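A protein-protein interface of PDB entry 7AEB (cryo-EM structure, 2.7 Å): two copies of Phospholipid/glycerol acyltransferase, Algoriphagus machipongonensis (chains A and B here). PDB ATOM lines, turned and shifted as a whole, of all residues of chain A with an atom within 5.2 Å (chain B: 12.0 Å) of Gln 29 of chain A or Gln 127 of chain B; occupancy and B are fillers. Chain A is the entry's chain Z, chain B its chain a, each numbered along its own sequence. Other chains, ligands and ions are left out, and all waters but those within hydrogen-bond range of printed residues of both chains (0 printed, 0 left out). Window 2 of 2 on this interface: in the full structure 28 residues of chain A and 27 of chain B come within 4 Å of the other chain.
N of Ala 126 of chain B lies within hydrogen-bond range of O of Gln 29 of chain A (3.2 Å).
NE2 of Gln 127 of chain B sits close to NE2 of Gln 29 of chain A (3.4 Å).
The side-chain hydroxyl (OG) of Ser 30 of chain A lies within hydrogen-bond range of the backbone carbonyl oxygen (O) of Phe 124 of chain B (3.1 Å).
N of Phe 124 of chain B lies within hydrogen-bond range of O of Val 31 of chain A (3.4 Å).
N of Gln 29 of chain A is in hydrogen-bond range of O of Lys 67 of chain A (2.8 Å).
N of Lys 67 of chain A lies within hydrogen-bond range of O of Ser 30 of chain A (3.1 Å).
The backbone NH (N) of Gln 127 of chain B is in hydrogen-bond range of the side-chain amide oxygen (OD1) of Asn 125 of chain B (2.9 Å).
Among the printed residues, merely in contact across the chains: Phe 12 of chain A with Phe 124 of chain B (3.8 Å) and Val 31 of chain A with Asp 123 of chain B (3.9 Å).
Gln 29 of chain A touches just these residues of chain B: Ala 126 (3.2 Å) and Gln 127 (3.4 Å).
Gln 127 of chain B touches just one residue of chain A: Gln 29 (3.4 Å).
No residue of chain B comes within 4 Å of Phe 28 of chain A.
Ser 30 of chain A touches just one residue of chain B: Phe 124.
No residue of chain B comes within 4 Å of Lys 67 of chain A.
No residue of chain B comes within 4 Å of Gly 69 of chain A.
No residue of chain B comes within 4 Å of Ile 133 of chain A.
Printed residues of chain A within 4 Å of Phe 124 of chain B: Phe 12 (3.8 Å), Ser 30 (3.1 Å) and Val 31 (3.4 Å).
Of the printed residues of chain A, Ala 126 of chain B touches Gln 29.
Of the printed residues of chain B, Val 31 of chain A touches Asp 123 and Phe 124.
Printed residues of chain A within 4 Å of Asp 123 of chain B: Val 31 (3.9 Å).
Lys 130 of chain B touches none of the printed residues of chain A.
The nearest residue of chain B that does not touch Gln 29 of chain A is Asn 125 of chain B (4.03 Å).
The nearest printed residue of chain A that does not touch Gln 127 of chain B is Phe 12 of chain A (6.6 Å).
Along chain A the printed residues that touch a printed residue of chain B span positions 12 to 31.
Of the 10 printed residues of chain B, 4 touch a printed residue of chain A.
Printed residues of chain B that touch a printed residue of chain A: Asp 123, Phe 124, Ala 126 and Gln 127.
Among the printed residues, 6 pairs touch across the chains.
Among the printed residues, no Asp or Glu carboxylate lies within 4 Å of a Lys or Arg side-chain nitrogen of the other chain.
No position is printed for both chains.
Of the 6 pairs that touch across the chains among the printed residues, none has its exchanged pair printed and touching as well.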
ATOM      1  N   PHE A  12      12.486 -25.649 -11.645  1.00  0.00           N
ATOM      2  CA  PHE A  12      11.411 -26.642 -11.616  1.00  0.00           C
ATOM      3  C   PHE A  12      11.737 -27.853 -10.730  1.00  0.00           C
ATOM      4  O   PHE A  12      12.899 -28.131 -10.439  1.00  0.00           O
ATOM      5  CB  PHE A  12      11.108 -27.115 -13.044  1.00  0.00           C
ATOM      6  CG  PHE A  12      12.311 -27.696 -13.762  1.00  0.00           C
ATOM      7  CD1 PHE A  12      12.622 -29.042 -13.684  1.00  0.00           C
ATOM      8  CD2 PHE A  12      13.134 -26.887 -14.518  1.00  0.00           C
ATOM      9  CE1 PHE A  12      13.742 -29.546 -14.317  1.00  0.00           C
ATOM     10  CE2 PHE A  12      14.235 -27.399 -15.161  1.00  0.00           C
ATOM     11  CZ  PHE A  12      14.531 -28.733 -15.064  1.00  0.00           C
ATOM     12  N   GLU A  27      15.732 -34.188  -8.376  1.00  0.00           N
ATOM     13  CA  GLU A  27      16.521 -33.193  -9.086  1.00  0.00           C
ATOM     14  C   GLU A  27      16.908 -33.653 -10.484  1.00  0.00           C
ATOM     15  O   GLU A  27      17.588 -34.666 -10.643  1.00  0.00           O
ATOM     16  CB  GLU A  27      17.760 -32.876  -8.271  1.00  0.00           C
ATOM     17  CG  GLU A  27      17.445 -32.743  -6.808  1.00  0.00           C
ATOM     18  CD  GLU A  27      18.674 -32.822  -5.954  1.00  0.00           C
ATOM     19  OE1 GLU A  27      19.732 -33.201  -6.495  1.00  0.00           O
ATOM     20  OE2 GLU A  27      18.584 -32.509  -4.748  1.00  0.00           O
ATOM     21  N   PHE A  28      16.527 -32.871 -11.489  1.00  0.00           N
ATOM     22  CA  PHE A  28      16.793 -33.236 -12.867  1.00  0.00           C
ATOM     23  C   PHE A  28      17.407 -32.092 -13.651  1.00  0.00           C
ATOM     24  O   PHE A  28      17.235 -30.921 -13.333  1.00  0.00           O
ATOM     25  CB  PHE A  28      15.524 -33.734 -13.542  1.00  0.00           C
ATOM     26  CG  PHE A  28      15.129 -35.103 -13.107  1.00  0.00           C
ATOM     27  CD1 PHE A  28      14.236 -35.288 -12.062  1.00  0.00           C
ATOM     28  CD2 PHE A  28      15.684 -36.207 -13.708  1.00  0.00           C
ATOM     29  CE1 PHE A  28      13.895 -36.552 -11.649  1.00  0.00           C
ATOM     30  CE2 PHE A  28      15.347 -37.467 -13.298  1.00  0.00           C
ATOM     31  CZ  PHE A  28      14.453 -37.640 -12.268  1.00  0.00           C
ATOM     32  N   GLN A  29      18.205 -32.486 -14.640  1.00  0.00           N
ATOM     33  CA  GLN A  29      18.819 -31.565 -15.594  1.00  0.00           C
ATOM     34  C   GLN A  29      17.812 -31.049 -16.620  1.00  0.00           C
ATOM     35  O   GLN A  29      17.866 -29.868 -17.004  1.00  0.00           O
ATOM     36  CB  GLN A  29      19.979 -32.265 -16.304  1.00  0.00           C
ATOM     37  CG  GLN A  29      20.652 -31.427 -17.372  1.00  0.00           C
ATOM     38  CD  GLN A  29      21.768 -32.156 -18.082  1.00  0.00           C
ATOM     39  OE1 GLN A  29      22.098 -33.289 -17.744  1.00  0.00           O
ATOM     40  NE2 GLN A  29      22.362 -31.503 -19.075  1.00  0.00           N
ATOM     41  N   SER A  30      16.895 -31.920 -17.079  1.00  0.00           N
ATOM     42  CA  SER A  30      15.967 -31.517 -18.124  1.00  0.00           C
ATOM     43  C   SER A  30      14.710 -32.402 -18.121  1.00  0.00           C
ATOM     44  O   SER A  30      14.758 -33.591 -17.789  1.00  0.00           O
ATOM     45  CB  SER A  30      16.643 -31.601 -19.481  1.00  0.00           C
ATOM     46  OG  SER A  30      15.699 -31.404 -20.491  1.00  0.00           O
ATOM     47  N   VAL A  31      13.583 -31.797 -18.514  1.00  0.00           N
ATOM     48  CA  VAL A  31      12.274 -32.456 -18.613  1.00  0.00           C
ATOM     49  C   VAL A  31      11.681 -32.167 -19.985  1.00  0.00           C
ATOM     50  O   VAL A  31      11.658 -31.013 -20.398  1.00  0.00           O
ATOM     51  CB  VAL A  31      11.269 -31.933 -17.570  1.00  0.00           C
ATOM     52  CG1 VAL A  31      10.095 -32.879 -17.437  1.00  0.00           C
ATOM     53  CG2 VAL A  31      11.901 -31.645 -16.272  1.00  0.00           C
ATOM     54  N   LYS A  67      16.222 -36.300 -17.767  1.00  0.00           N
ATOM     55  CA  LYS A  67      17.679 -36.463 -17.773  1.00  0.00           C
ATOM     56  C   LYS A  67      18.342 -35.904 -16.520  1.00  0.00           C
ATOM     57  O   LYS A  67      17.878 -34.916 -15.945  1.00  0.00           O
ATOM     58  CB  LYS A  67      18.323 -35.787 -18.971  1.00  0.00           C
ATOM     59  CG  LYS A  67      17.976 -36.409 -20.277  1.00  0.00           C
ATOM     60  CD  LYS A  67      18.707 -35.729 -21.399  1.00  0.00           C
ATOM     61  CE  LYS A  67      18.372 -36.356 -22.733  1.00  0.00           C
ATOM     62  NZ  LYS A  67      19.034 -35.642 -23.863  1.00  0.00           N
ATOM     63  N   ARG A  68      19.466 -36.525 -16.134  1.00  0.00           N
ATOM     64  CA  ARG A  68      20.276 -36.113 -14.984  1.00  0.00           C
ATOM     65  C   ARG A  68      21.651 -36.781 -15.012  1.00  0.00           C
ATOM     66  O   ARG A  68      21.881 -37.714 -15.777  1.00  0.00           O
ATOM     67  CB  ARG A  68      19.590 -36.479 -13.685  1.00  0.00           C
ATOM     68  CG  ARG A  68      19.472 -37.959 -13.513  1.00  0.00           C
ATOM     69  CD  ARG A  68      18.830 -38.285 -12.253  1.00  0.00           C
ATOM     70  NE  ARG A  68      18.849 -39.715 -12.060  1.00  0.00           N
ATOM     71  CZ  ARG A  68      18.244 -40.354 -11.075  1.00  0.00           C
ATOM     72  NH1 ARG A  68      17.535 -39.704 -10.165  1.00  0.00           N
ATOM     73  NH2 ARG A  68      18.371 -41.661 -11.021  1.00  0.00           N
ATOM     74  N   GLY A  69      22.554 -36.324 -14.135  1.00  0.00           N
ATOM     75  CA  GLY A  69      23.822 -37.027 -13.957  1.00  0.00           C
ATOM     76  C   GLY A  69      23.589 -38.363 -13.282  1.00  0.00           C
ATOM     77  O   GLY A  69      22.637 -38.521 -12.529  1.00  0.00           O
ATOM     78  N   ILE A 133      25.963 -39.172 -18.061  1.00  0.00           N
ATOM     79  CA  ILE A 133      24.562 -38.754 -18.076  1.00  0.00           C
ATOM     80  C   ILE A 133      23.617 -39.937 -18.259  1.00  0.00           C
ATOM     81  O   ILE A 133      23.797 -40.778 -19.155  1.00  0.00           O
ATOM     82  CB  ILE A 133      24.304 -37.685 -19.152  1.00  0.00           C
ATOM     83  CG1 ILE A 133      25.212 -36.456 -18.925  1.00  0.00           C
ATOM     84  CG2 ILE A 133      22.817 -37.277 -19.210  1.00  0.00           C
ATOM     85  CD1 ILE A 133      25.064 -35.729 -17.588  1.00  0.00           C
ATOM     86  N   GLU B 122       7.469 -25.671 -24.760  1.00  0.00           N
ATOM     87  CA  GLU B 122       8.837 -26.112 -25.028  1.00  0.00           C
ATOM     88  C   GLU B 122       9.567 -26.605 -23.775  1.00  0.00           C
ATOM     89  O   GLU B 122       9.272 -26.194 -22.652  1.00  0.00           O
ATOM     90  CB  GLU B 122       9.632 -24.981 -25.680  1.00  0.00           C
ATOM     91  CG  GLU B 122       9.121 -24.632 -27.061  1.00  0.00           C
ATOM     92  CD  GLU B 122       9.984 -23.658 -27.795  1.00  0.00           C
ATOM     93  OE1 GLU B 122      10.929 -23.138 -27.204  1.00  0.00           O
ATOM     94  OE2 GLU B 122       9.658 -23.337 -28.942  1.00  0.00           O
ATOM     95  N   ASP B 123      10.557 -27.477 -24.005  1.00  0.00           N
ATOM     96  CA  ASP B 123      11.347 -28.160 -22.976  1.00  0.00           C
ATOM     97  C   ASP B 123      12.032 -27.224 -21.984  1.00  0.00           C
ATOM     98  O   ASP B 123      12.536 -26.156 -22.334  1.00  0.00           O
ATOM     99  CB  ASP B 123      12.474 -28.973 -23.603  1.00  0.00           C
ATOM    100  CG  ASP B 123      12.016 -30.181 -24.364  1.00  0.00           C
ATOM    101  OD1 ASP B 123      10.848 -30.547 -24.327  1.00  0.00           O
ATOM    102  OD2 ASP B 123      12.867 -30.781 -25.021  1.00  0.00           O
ATOM    103  N   PHE B 124      12.127 -27.698 -20.754  1.00  0.00           N
ATOM    104  CA  PHE B 124      12.797 -26.991 -19.680  1.00  0.00           C
ATOM    105  C   PHE B 124      14.260 -27.407 -19.656  1.00  0.00           C
ATOM    106  O   PHE B 124      14.579 -28.560 -19.932  1.00  0.00           O
ATOM    107  CB  PHE B 124      12.143 -27.331 -18.345  1.00  0.00           C
ATOM    108  CG  PHE B 124      10.687 -26.935 -18.235  1.00  0.00           C
ATOM    109  CD1 PHE B 124       9.904 -27.533 -17.278  1.00  0.00           C
ATOM    110  CD2 PHE B 124      10.094 -25.988 -19.069  1.00  0.00           C
ATOM    111  CE1 PHE B 124       8.573 -27.209 -17.145  1.00  0.00           C
ATOM    112  CE2 PHE B 124       8.762 -25.673 -18.940  1.00  0.00           C
ATOM    113  CZ  PHE B 124       8.006 -26.283 -17.973  1.00  0.00           C
ATOM    114  N   ASN B 125      15.148 -26.472 -19.325  1.00  0.00           N
ATOM    115  CA  ASN B 125      16.577 -26.786 -19.263  1.00  0.00           C
ATOM    116  C   ASN B 125      17.222 -25.978 -18.147  1.00  0.00           C
ATOM    117  O   ASN B 125      17.341 -24.759 -18.233  1.00  0.00           O
ATOM    118  CB  ASN B 125      17.245 -26.526 -20.605  1.00  0.00           C
ATOM    119  CG  ASN B 125      18.691 -27.001 -20.661  1.00  0.00           C
ATOM    120  OD1 ASN B 125      19.439 -27.029 -19.678  1.00  0.00           O
ATOM    121  ND2 ASN B 125      19.097 -27.373 -21.846  1.00  0.00           N
ATOM    122  N   ALA B 126      17.694 -26.695 -17.129  1.00  0.00           N
ATOM    123  CA  ALA B 126      18.289 -26.107 -15.938  1.00  0.00           C
ATOM    124  C   ALA B 126      19.562 -25.324 -16.209  1.00  0.00           C
ATOM    125  O   ALA B 126      19.981 -24.527 -15.367  1.00  0.00           O
ATOM    126  CB  ALA B 126      18.610 -27.206 -14.944  1.00  0.00           C
ATOM    127  N   GLN B 127      20.221 -25.579 -17.332  1.00  0.00           N
ATOM    128  CA  GLN B 127      21.488 -24.941 -17.641  1.00  0.00           C
ATOM    129  C   GLN B 127      21.384 -23.843 -18.697  1.00  0.00           C
ATOM    130  O   GLN B 127      22.419 -23.363 -19.166  1.00  0.00           O
ATOM    131  CB  GLN B 127      22.495 -25.998 -18.079  1.00  0.00           C
ATOM    132  CG  GLN B 127      22.835 -26.973 -16.972  1.00  0.00           C
ATOM    133  CD  GLN B 127      23.836 -28.012 -17.381  1.00  0.00           C
ATOM    134  OE1 GLN B 127      24.783 -27.726 -18.108  1.00  0.00           O
ATOM    135  NE2 GLN B 127      23.638 -29.233 -16.916  1.00  0.00           N
ATOM    136  N   GLU B 128      20.180 -23.411 -19.073  1.00  0.00           N
ATOM    137  CA  GLU B 128      20.065 -22.381 -20.092  1.00  0.00           C
ATOM    138  C   GLU B 128      19.175 -21.243 -19.594  1.00  0.00           C
ATOM    139  O   GLU B 128      18.214 -21.462 -18.860  1.00  0.00           O
ATOM    140  CB  GLU B 128      19.451 -22.960 -21.353  1.00  0.00           C
ATOM    141  CG  GLU B 128      20.349 -23.899 -22.124  1.00  0.00           C
ATOM    142  CD  GLU B 128      19.689 -24.381 -23.385  1.00  0.00           C
ATOM    143  OE1 GLU B 128      18.458 -24.371 -23.452  1.00  0.00           O
ATOM    144  OE2 GLU B 128      20.395 -24.716 -24.342  1.00  0.00           O
ATOM    145  N   SER B 129      19.481 -20.031 -20.005  1.00  0.00           N
ATOM    146  CA  SER B 129      18.642 -18.869 -19.717  1.00  0.00           C
ATOM    147  C   SER B 129      17.670 -18.580 -20.836  1.00  0.00           C
ATOM    148  O   SER B 129      18.048 -18.003 -21.854  1.00  0.00           O
ATOM    149  CB  SER B 129      19.511 -17.656 -19.459  1.00  0.00           C
ATOM    150  OG  SER B 129      18.718 -16.578 -19.048  1.00  0.00           O
ATOM    151  N   LYS B 130      16.410 -18.984 -20.652  1.00  0.00           N
ATOM    152  CA  LYS B 130      15.396 -18.888 -21.694  1.00  0.00           C
ATOM    153  C   LYS B 130      14.013 -18.636 -21.108  1.00  0.00           C
ATOM    154  O   LYS B 130      13.734 -18.964 -19.958  1.00  0.00           O
ATOM    155  CB  LYS B 130      15.357 -20.173 -22.516  1.00  0.00           C
ATOM    156  CG  LYS B 130      16.523 -20.367 -23.443  1.00  0.00           C
ATOM    157  CD  LYS B 130      16.388 -21.610 -24.259  1.00  0.00           C
ATOM    158  CE  LYS B 130      17.636 -21.842 -25.094  1.00  0.00           C
ATOM    159  NZ  LYS B 130      17.598 -23.157 -25.793  1.00  0.00           N
ATOM    160  N   MET B 131      13.142 -18.079 -21.940  1.00  0.00           N
ATOM    161  CA  MET B 131      11.745 -17.856 -21.595  1.00  0.00           C
ATOM    162  C   MET B 131      10.927 -19.095 -21.921  1.00  0.00           C
ATOM    163  O   MET B 131      11.190 -19.767 -22.915  1.00  0.00           O
ATOM    164  CB  MET B 131      11.218 -16.660 -22.380  1.00  0.00           C
ATOM    165  CG  MET B 131       9.797 -16.277 -22.088  1.00  0.00           C
ATOM    166  SD  MET B 131       9.280 -14.836 -22.995  1.00  0.00           S
ATOM    167  CE  MET B 131      10.094 -13.523 -22.098  1.00  0.00           C
